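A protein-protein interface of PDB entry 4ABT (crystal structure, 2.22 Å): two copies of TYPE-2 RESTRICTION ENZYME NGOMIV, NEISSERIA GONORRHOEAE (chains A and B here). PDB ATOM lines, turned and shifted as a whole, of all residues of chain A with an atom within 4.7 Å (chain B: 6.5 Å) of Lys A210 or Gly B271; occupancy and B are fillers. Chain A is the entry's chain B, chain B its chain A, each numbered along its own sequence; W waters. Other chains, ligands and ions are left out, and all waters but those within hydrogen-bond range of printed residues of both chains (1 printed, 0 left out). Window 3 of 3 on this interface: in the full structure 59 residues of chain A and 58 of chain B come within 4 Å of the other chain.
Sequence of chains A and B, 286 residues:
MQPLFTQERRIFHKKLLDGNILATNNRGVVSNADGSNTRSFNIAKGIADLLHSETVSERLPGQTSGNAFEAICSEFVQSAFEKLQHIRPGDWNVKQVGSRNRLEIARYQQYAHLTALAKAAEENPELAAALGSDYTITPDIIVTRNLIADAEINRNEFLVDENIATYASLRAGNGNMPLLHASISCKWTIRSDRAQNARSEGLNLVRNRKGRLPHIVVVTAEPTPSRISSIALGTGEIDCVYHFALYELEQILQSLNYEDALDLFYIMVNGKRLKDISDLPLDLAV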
ATOM      1  N   GLN A 110      10.935 -19.317 -19.311  1.00  0.00           N
ATOM      2  CA  GLN A 110       9.676 -18.731 -18.809  1.00  0.00           C
ATOM      3  C   GLN A 110       9.075 -19.459 -17.602  1.00  0.00           C
ATOM      4  O   GLN A 110       8.157 -18.955 -16.940  1.00  0.00           O
ATOM      5  CB  GLN A 110       8.628 -18.743 -19.919  1.00  0.00           C
ATOM      6  CG  GLN A 110       9.034 -18.039 -21.177  1.00  0.00           C
ATOM      7  CD  GLN A 110       9.480 -18.979 -22.281  1.00  0.00           C
ATOM      8  OE1 GLN A 110      10.524 -19.673 -22.170  1.00  0.00           O
ATOM      9  NE2 GLN A 110       8.738 -18.964 -23.393  1.00  0.00           N
ATOM     10  N   HIS A 113      11.346 -20.902 -12.712  1.00  0.00           N
ATOM     11  CA  HIS A 113      11.050 -20.628 -11.330  1.00  0.00           C
ATOM     12  C   HIS A 113      10.222 -21.754 -10.733  1.00  0.00           C
ATOM     13  O   HIS A 113      10.109 -21.851  -9.523  1.00  0.00           O
ATOM     14  CB  HIS A 113      10.316 -19.301 -11.184  1.00  0.00           C
ATOM     15  CG  HIS A 113       8.992 -19.270 -11.878  1.00  0.00           C
ATOM     16  ND1 HIS A 113       8.880 -19.277 -13.251  1.00  0.00           N
ATOM     17  CD2 HIS A 113       7.727 -19.235 -11.400  1.00  0.00           C
ATOM     18  CE1 HIS A 113       7.604 -19.240 -13.591  1.00  0.00           C
ATOM     19  NE2 HIS A 113       6.883 -19.214 -12.487  1.00  0.00           N
ATOM     20  N   ASN A 208       1.454 -19.147 -15.522  1.00  0.00           N
ATOM     21  CA  ASN A 208       2.733 -19.239 -14.811  1.00  0.00           C
ATOM     22  C   ASN A 208       3.967 -18.681 -15.490  1.00  0.00           C
ATOM     23  O   ASN A 208       5.063 -18.782 -14.947  1.00  0.00           O
ATOM     24  CB  ASN A 208       3.005 -20.693 -14.496  1.00  0.00           C
ATOM     25  CG  ASN A 208       2.014 -21.204 -13.538  1.00  0.00           C
ATOM     26  OD1 ASN A 208       1.951 -20.728 -12.405  1.00  0.00           O
ATOM     27  ND2 ASN A 208       1.129 -22.061 -14.014  1.00  0.00           N
ATOM     28  N   ARG A 209       3.774 -18.129 -16.673  1.00  0.00           N
ATOM     29  CA  ARG A 209       4.858 -17.703 -17.519  1.00  0.00           C
ATOM     30  C   ARG A 209       5.485 -16.444 -16.954  1.00  0.00           C
ATOM     31  O   ARG A 209       4.771 -15.531 -16.528  1.00  0.00           O
ATOM     32  CB  ARG A 209       4.339 -17.407 -18.976  1.00  0.00           C
ATOM     33  CG  ARG A 209       3.554 -16.073 -19.115  1.00  0.00           C
ATOM     34  CD  ARG A 209       2.994 -15.842 -20.537  1.00  0.00           C
ATOM     35  NE  ARG A 209       2.558 -14.446 -20.742  1.00  0.00           N
ATOM     36  CZ  ARG A 209       1.351 -14.011 -20.400  1.00  0.00           C
ATOM     37  NH1 ARG A 209       0.487 -14.867 -19.891  1.00  0.00           N
ATOM     38  NH2 ARG A 209       0.996 -12.748 -20.566  1.00  0.00           N
ATOM     39  N   LYS A 210       6.810 -16.406 -17.019  1.00  0.00           N
ATOM     40  CA  LYS A 210       7.584 -15.160 -16.976  1.00  0.00           C
ATOM     41  C   LYS A 210       8.230 -14.868 -18.341  1.00  0.00           C
ATOM     42  O   LYS A 210       9.246 -15.469 -18.681  1.00  0.00           O
ATOM     43  CB  LYS A 210       8.638 -15.257 -15.906  1.00  0.00           C
ATOM     44  CG  LYS A 210       8.004 -15.575 -14.525  1.00  0.00           C
ATOM     45  CD  LYS A 210       9.042 -15.479 -13.448  1.00  0.00           C
ATOM     46  CE  LYS A 210       8.405 -15.747 -12.130  1.00  0.00           C
ATOM     47  NZ  LYS A 210       9.396 -15.509 -11.088  1.00  0.00           N
ATOM     48  N   GLY A 211       7.630 -13.965 -19.115  1.00  0.00           N
ATOM     49  CA  GLY A 211       8.095 -13.647 -20.480  1.00  0.00           C
ATOM     50  C   GLY A 211       7.018 -14.034 -21.509  1.00  0.00           C
ATOM     51  O   GLY A 211       5.861 -14.239 -21.150  1.00  0.00           O
ATOM     52  N   ARG A 212       7.393 -14.127 -22.780  1.00  0.00           N
ATOM     53  CA  ARG A 212       6.441 -14.331 -23.863  1.00  0.00           C
ATOM     54  C   ARG A 212       5.880 -15.738 -23.807  1.00  0.00           C
ATOM     55  O   ARG A 212       6.638 -16.716 -23.637  1.00  0.00           O
ATOM     56  CB  ARG A 212       7.060 -14.098 -25.260  1.00  0.00           C
ATOM     57  CG  ARG A 212       5.923 -13.905 -26.310  1.00  0.00           C
ATOM     58  CD  ARG A 212       6.214 -14.206 -27.770  1.00  0.00           C
ATOM     59  NE  ARG A 212       5.051 -13.844 -28.623  1.00  0.00           N
ATOM     60  CZ  ARG A 212       5.096 -13.619 -29.961  1.00  0.00           C
ATOM     61  NH1 ARG A 212       6.251 -13.711 -30.636  1.00  0.00           N
ATOM     62  NH2 ARG A 212       3.984 -13.309 -30.651  1.00  0.00           N
ATOM     63  N   GLY B 234       3.577 -10.988  -9.810  1.00  0.00           N
ATOM     64  CA  GLY B 234       2.562 -11.869 -10.355  1.00  0.00           C
ATOM     65  C   GLY B 234       2.873 -12.201 -11.803  1.00  0.00           C
ATOM     66  O   GLY B 234       3.719 -11.544 -12.456  1.00  0.00           O
ATOM     67  N   THR B 235       2.165 -13.214 -12.290  1.00  0.00           N
ATOM     68  CA  THR B 235       2.321 -13.748 -13.607  1.00  0.00           C
ATOM     69  C   THR B 235       0.945 -14.046 -14.160  1.00  0.00           C
ATOM     70  O   THR B 235      -0.018 -14.285 -13.421  1.00  0.00           O
ATOM     71  CB  THR B 235       3.237 -15.049 -13.660  1.00  0.00           C
ATOM     72  OG1 THR B 235       2.667 -16.117 -12.886  1.00  0.00           O
ATOM     73  CG2 THR B 235       4.627 -14.753 -13.182  1.00  0.00           C
ATOM     74  N   ILE B 238       0.847  -9.926 -17.536  1.00  0.00           N
ATOM     75  CA  ILE B 238       1.985  -9.212 -18.058  1.00  0.00           C
ATOM     76  C   ILE B 238       3.202 -10.129 -18.223  1.00  0.00           C
ATOM     77  O   ILE B 238       3.585 -10.811 -17.284  1.00  0.00           O
ATOM     78  CB  ILE B 238       2.345  -8.053 -17.104  1.00  0.00           C
ATOM     79  CG1 ILE B 238       1.100  -7.258 -16.667  1.00  0.00           C
ATOM     80  CG2 ILE B 238       3.461  -7.190 -17.717  1.00  0.00           C
ATOM     81  CD1 ILE B 238       0.251  -6.727 -17.788  1.00  0.00           C
ATOM     82  N   ASP B 239       3.807 -10.156 -19.423  1.00  0.00           N
ATOM     83  CA  ASP B 239       5.045 -10.931 -19.627  1.00  0.00           C
ATOM     84  C   ASP B 239       6.197 -10.422 -18.790  1.00  0.00           C
ATOM     85  O   ASP B 239       6.919 -11.239 -18.152  1.00  0.00           O
ATOM     86  CB  ASP B 239       5.483 -10.891 -21.081  1.00  0.00           C
ATOM     87  CG  ASP B 239       4.450 -11.459 -22.022  1.00  0.00           C
ATOM     88  OD1 ASP B 239       3.407 -11.960 -21.545  1.00  0.00           O
ATOM     89  OD2 ASP B 239       4.654 -11.311 -23.250  1.00  0.00           O
ATOM     90  N   CYS B 240       6.408  -9.094 -18.833  1.00  0.00           N
ATOM     91  CA  CYS B 240       7.472  -8.458 -18.022  1.00  0.00           C
ATOM     92  C   CYS B 240       7.298  -6.927 -17.959  1.00  0.00           C
ATOM     93  O   CYS B 240       6.683  -6.321 -18.868  1.00  0.00           O
ATOM     94  CB  CYS B 240       8.850  -8.814 -18.585  1.00  0.00           C
ATOM     95  SG  CYS B 240      10.259  -8.338 -17.529  1.00  0.00           S
ATOM     96  N   PHE B 265      13.272  -4.480  -5.166  1.00  0.00           N
ATOM     97  CA  PHE B 265      13.937  -4.371  -6.463  1.00  0.00           C
ATOM     98  C   PHE B 265      14.470  -5.752  -6.874  1.00  0.00           C
ATOM     99  O   PHE B 265      14.197  -6.194  -7.986  1.00  0.00           O
ATOM    100  CB  PHE B 265      15.039  -3.310  -6.402  1.00  0.00           C
ATOM    101  CG  PHE B 265      15.784  -3.113  -7.677  1.00  0.00           C
ATOM    102  CD1 PHE B 265      16.933  -3.864  -7.966  1.00  0.00           C
ATOM    103  CD2 PHE B 265      15.363  -2.188  -8.614  1.00  0.00           C
ATOM    104  CE1 PHE B 265      17.631  -3.693  -9.184  1.00  0.00           C
ATOM    105  CE2 PHE B 265      16.098  -2.003  -9.831  1.00  0.00           C
ATOM    106  CZ  PHE B 265      17.223  -2.743 -10.094  1.00  0.00           C
ATOM    107  N   TYR B 266      15.154  -6.472  -5.979  1.00  0.00           N
ATOM    108  CA  TYR B 266      15.760  -7.711  -6.409  1.00  0.00           C
ATOM    109  C   TYR B 266      14.726  -8.801  -6.516  1.00  0.00           C
ATOM    110  O   TYR B 266      14.820  -9.644  -7.376  1.00  0.00           O
ATOM    111  CB  TYR B 266      16.936  -8.146  -5.520  1.00  0.00           C
ATOM    112  CG  TYR B 266      18.129  -7.291  -5.798  1.00  0.00           C
ATOM    113  CD1 TYR B 266      18.645  -7.180  -7.098  1.00  0.00           C
ATOM    114  CD2 TYR B 266      18.709  -6.532  -4.784  1.00  0.00           C
ATOM    115  CE1 TYR B 266      19.760  -6.353  -7.365  1.00  0.00           C
ATOM    116  CE2 TYR B 266      19.822  -5.705  -5.040  1.00  0.00           C
ATOM    117  CZ  TYR B 266      20.326  -5.628  -6.314  1.00  0.00           C
ATOM    118  OH  TYR B 266      21.382  -4.803  -6.526  1.00  0.00           O
ATOM    119  N   ILE B 267      13.717  -8.777  -5.662  1.00  0.00           N
ATOM    120  CA  ILE B 267      12.682  -9.755  -5.812  1.00  0.00           C
ATOM    121  C   ILE B 267      12.203  -9.644  -7.279  1.00  0.00           C
ATOM    122  O   ILE B 267      12.087 -10.648  -7.964  1.00  0.00           O
ATOM    123  CB  ILE B 267      11.534  -9.556  -4.834  1.00  0.00           C
ATOM    124  CG1 ILE B 267      11.982  -9.898  -3.415  1.00  0.00           C
ATOM    125  CG2 ILE B 267      10.302 -10.438  -5.212  1.00  0.00           C
ATOM    126  CD1 ILE B 267      10.853  -9.888  -2.421  1.00  0.00           C
ATOM    127  N   MET B 268      11.994  -8.414  -7.749  1.00  0.00           N
ATOM    128  CA  MET B 268      11.391  -8.160  -9.059  1.00  0.00           C
ATOM    129  C   MET B 268      12.352  -8.489 -10.193  1.00  0.00           C
ATOM    130  O   MET B 268      11.963  -9.109 -11.191  1.00  0.00           O
ATOM    131  CB  MET B 268      10.931  -6.717  -9.156  1.00  0.00           C
ATOM    132  CG  MET B 268       9.659  -6.486  -8.388  1.00  0.00           C
ATOM    133  SD  MET B 268       8.950  -4.861  -8.648  1.00  0.00           S
ATOM    134  CE  MET B 268      10.162  -3.845  -7.778  1.00  0.00           C
ATOM    135  N   VAL B 269      13.605  -8.063 -10.023  1.00  0.00           N
ATOM    136  CA  VAL B 269      14.593  -8.182 -11.074  1.00  0.00           C
ATOM    137  C   VAL B 269      15.087  -9.636 -11.096  1.00  0.00           C
ATOM    138  O   VAL B 269      15.120 -10.270 -12.156  1.00  0.00           O
ATOM    139  CB  VAL B 269      15.730  -7.200 -10.881  1.00  0.00           C
ATOM    140  CG1 VAL B 269      16.934  -7.568 -11.785  1.00  0.00           C
ATOM    141  CG2 VAL B 269      15.242  -5.762 -11.105  1.00  0.00           C
ATOM    142  N   ASN B 270      15.443 -10.188  -9.929  1.00  0.00           N
ATOM    143  CA  ASN B 270      15.860 -11.598  -9.915  1.00  0.00           C
ATOM    144  C   ASN B 270      14.704 -12.561 -10.268  1.00  0.00           C
ATOM    145  O   ASN B 270      14.909 -13.646 -10.863  1.00  0.00           O
ATOM    146  CB  ASN B 270      16.626 -11.942  -8.616  1.00  0.00           C
ATOM    147  CG  ASN B 270      17.930 -11.116  -8.471  1.00  0.00           C
ATOM    148  OD1 ASN B 270      18.565 -10.728  -9.468  1.00  0.00           O
ATOM    149  ND2 ASN B 270      18.322 -10.843  -7.233  1.00  0.00           N
ATOM    150  N   GLY B 271      13.489 -12.150  -9.938  1.00  0.00           N
ATOM    151  CA  GLY B 271      12.295 -12.921 -10.290  1.00  0.00           C
ATOM    152  C   GLY B 271      11.811 -12.755 -11.732  1.00  0.00           C
ATOM    153  O   GLY B 271      10.763 -13.291 -12.061  1.00  0.00           O
ATOM    154  N   LYS B 272      12.550 -12.040 -12.578  1.00  0.00           N
ATOM    155  CA  LYS B 272      12.206 -11.901 -13.990  1.00  0.00           C
ATOM    156  C   LYS B 272      10.845 -11.195 -14.201  1.00  0.00           C
ATOM    157  O   LYS B 272      10.033 -11.621 -15.043  1.00  0.00           O
ATOM    158  CB  LYS B 272      12.225 -13.255 -14.706  1.00  0.00           C
ATOM    159  CG  LYS B 272      13.572 -13.965 -14.689  1.00  0.00           C
ATOM    160  CD  LYS B 272      13.514 -15.330 -15.409  1.00  0.00           C
ATOM    161  N   ARG B 273      10.575 -10.168 -13.376  1.00  0.00           N
ATOM    162  CA  ARG B 273       9.355  -9.391 -13.494  1.00  0.00           C
ATOM    163  C   ARG B 273       9.661  -7.967 -13.894  1.00  0.00           C
ATOM    164  O   ARG B 273       8.740  -7.196 -14.166  1.00  0.00           O
ATOM    165  CB  ARG B 273       8.591  -9.358 -12.177  1.00  0.00           C
ATOM    166  CG  ARG B 273       8.375 -10.748 -11.516  1.00  0.00           C
ATOM    167  CD  ARG B 273       7.731 -11.817 -12.428  1.00  0.00           C
ATOM    168  NE  ARG B 273       6.479 -11.427 -13.093  1.00  0.00           N
ATOM    169  CZ  ARG B 273       6.268 -11.406 -14.415  1.00  0.00           C
ATOM    170  NH1 ARG B 273       7.226 -11.740 -15.293  1.00  0.00           N
ATOM    171  NH2 ARG B 273       5.066 -11.079 -14.864  1.00  0.00           N
ATOM    172  N   LEU B 274      10.954  -7.612 -13.873  1.00  0.00           N
ATOM    173  CA  LEU B 274      11.435  -6.253 -14.108  1.00  0.00           C
ATOM    174  C   LEU B 274      12.845  -6.221 -14.750  1.00  0.00           C
ATOM    175  O   LEU B 274      13.788  -6.919 -14.337  1.00  0.00           O
ATOM    176  CB  LEU B 274      11.347  -5.418 -12.809  1.00  0.00           C
ATOM    177  CG  LEU B 274      11.800  -3.935 -12.884  1.00  0.00           C
ATOM    178  CD1 LEU B 274      10.775  -3.083 -13.606  1.00  0.00           C
ATOM    179  CD2 LEU B 274      12.122  -3.328 -11.483  1.00  0.00           C
HETATM  180  O   HOH W   1       3.101 -13.358 -17.077  1.00  0.00           O
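No position is printed for both chains. Of the 10 pairs that touch across the chains among the printed residues, none has its exchanged pair printed and touching as well.
The guanidinium group (NH2) of Arg A209 is in salt-bridge range of the side-chain carboxylate (OD1) of Asp B239, at 2.7 Å. NZ of Lys A210 sits at hydrogen-bond distance from O of Gly B271 (2.8 Å). The backbone carbonyl oxygen (O) of Asp B239 is in hydrogen-bond range of the backbone NH (N) of Gly A211 (3.0 Å).
Along chain A the printed residues that touch a printed residue of chain B span positions 208 to 212. Printed residues of chain B that touch a printed residue of chain A: Thr B235, Asp B239, Gly B271, Lys B272 and Arg B273. Among the printed residues, 10 pairs touch across the chains. Among the printed residues, Asp or Glu carboxylates within 4 Å of a Lys or Arg side-chain nitrogen of the other chain: Arg A209 with Asp B239.
Of the printed residues of chain B, Lys A210 touches Thr B235 (3.7 Å), Asp B239 (3.9 Å), Gly B271 (2.8 Å), Lys B272 (3.99 Å) and Arg B273 (3.8 Å). Printed residues of chain A within 4 Å of Gly B271: Lys A210. Of the printed residues of chain A, Arg B273 touches Lys A210 (3.8 Å). Printed residues of chain A within 4 Å of Asp B239: Arg A209, Lys A210, Gly A211 and Arg A212. Of the printed residues of chain B, Arg A212 touches Asp B239 (3.6 Å). Of the printed residues of chain B, Asn A208 touches Thr B235 (3.7 Å). Of the printed residues of chain B, Arg A209 touches Thr B235 and Asp B239. The nearest printed residue of chain A that does not touch Gly B271 is His A113 (6.1 Å).
Among the printed residues, pairs that only touch across the chains: Arg A209 with Thr B235, Arg A212 with Asp B239, Asn A208 with Thr B235, Lys A210 with Thr B235, Lys A210 with Arg B273, Lys A210 with Asp B239 and Lys A210 with Lys B272.
The backbone NH (N) of Lys A210 is in hydrogen-bond range of the backbone carbonyl oxygen (O) of Gln A110, 2.9 Å away. The backbone carbonyl oxygen (O) of Asn A208 sits close to a ring nitrogen (NE2) of His A113, at 3.1 Å. O of Gly B234 sits at hydrogen-bond distance from NH2 of Arg B273, 2.8 Å away. O of Asp B239 lies within hydrogen-bond range of NH1 of Arg B273 (2.9 Å). NE of Arg A209 sits at hydrogen-bond distance from O of Gly A211, 3.3 Å away. N of Arg B273 is in hydrogen-bond range of O of Met B268 (2.8 Å).
Water W1 lies within hydrogen-bond range of O of Ile B238 (2.6 Å) and O of Arg A209 (2.8 Å).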
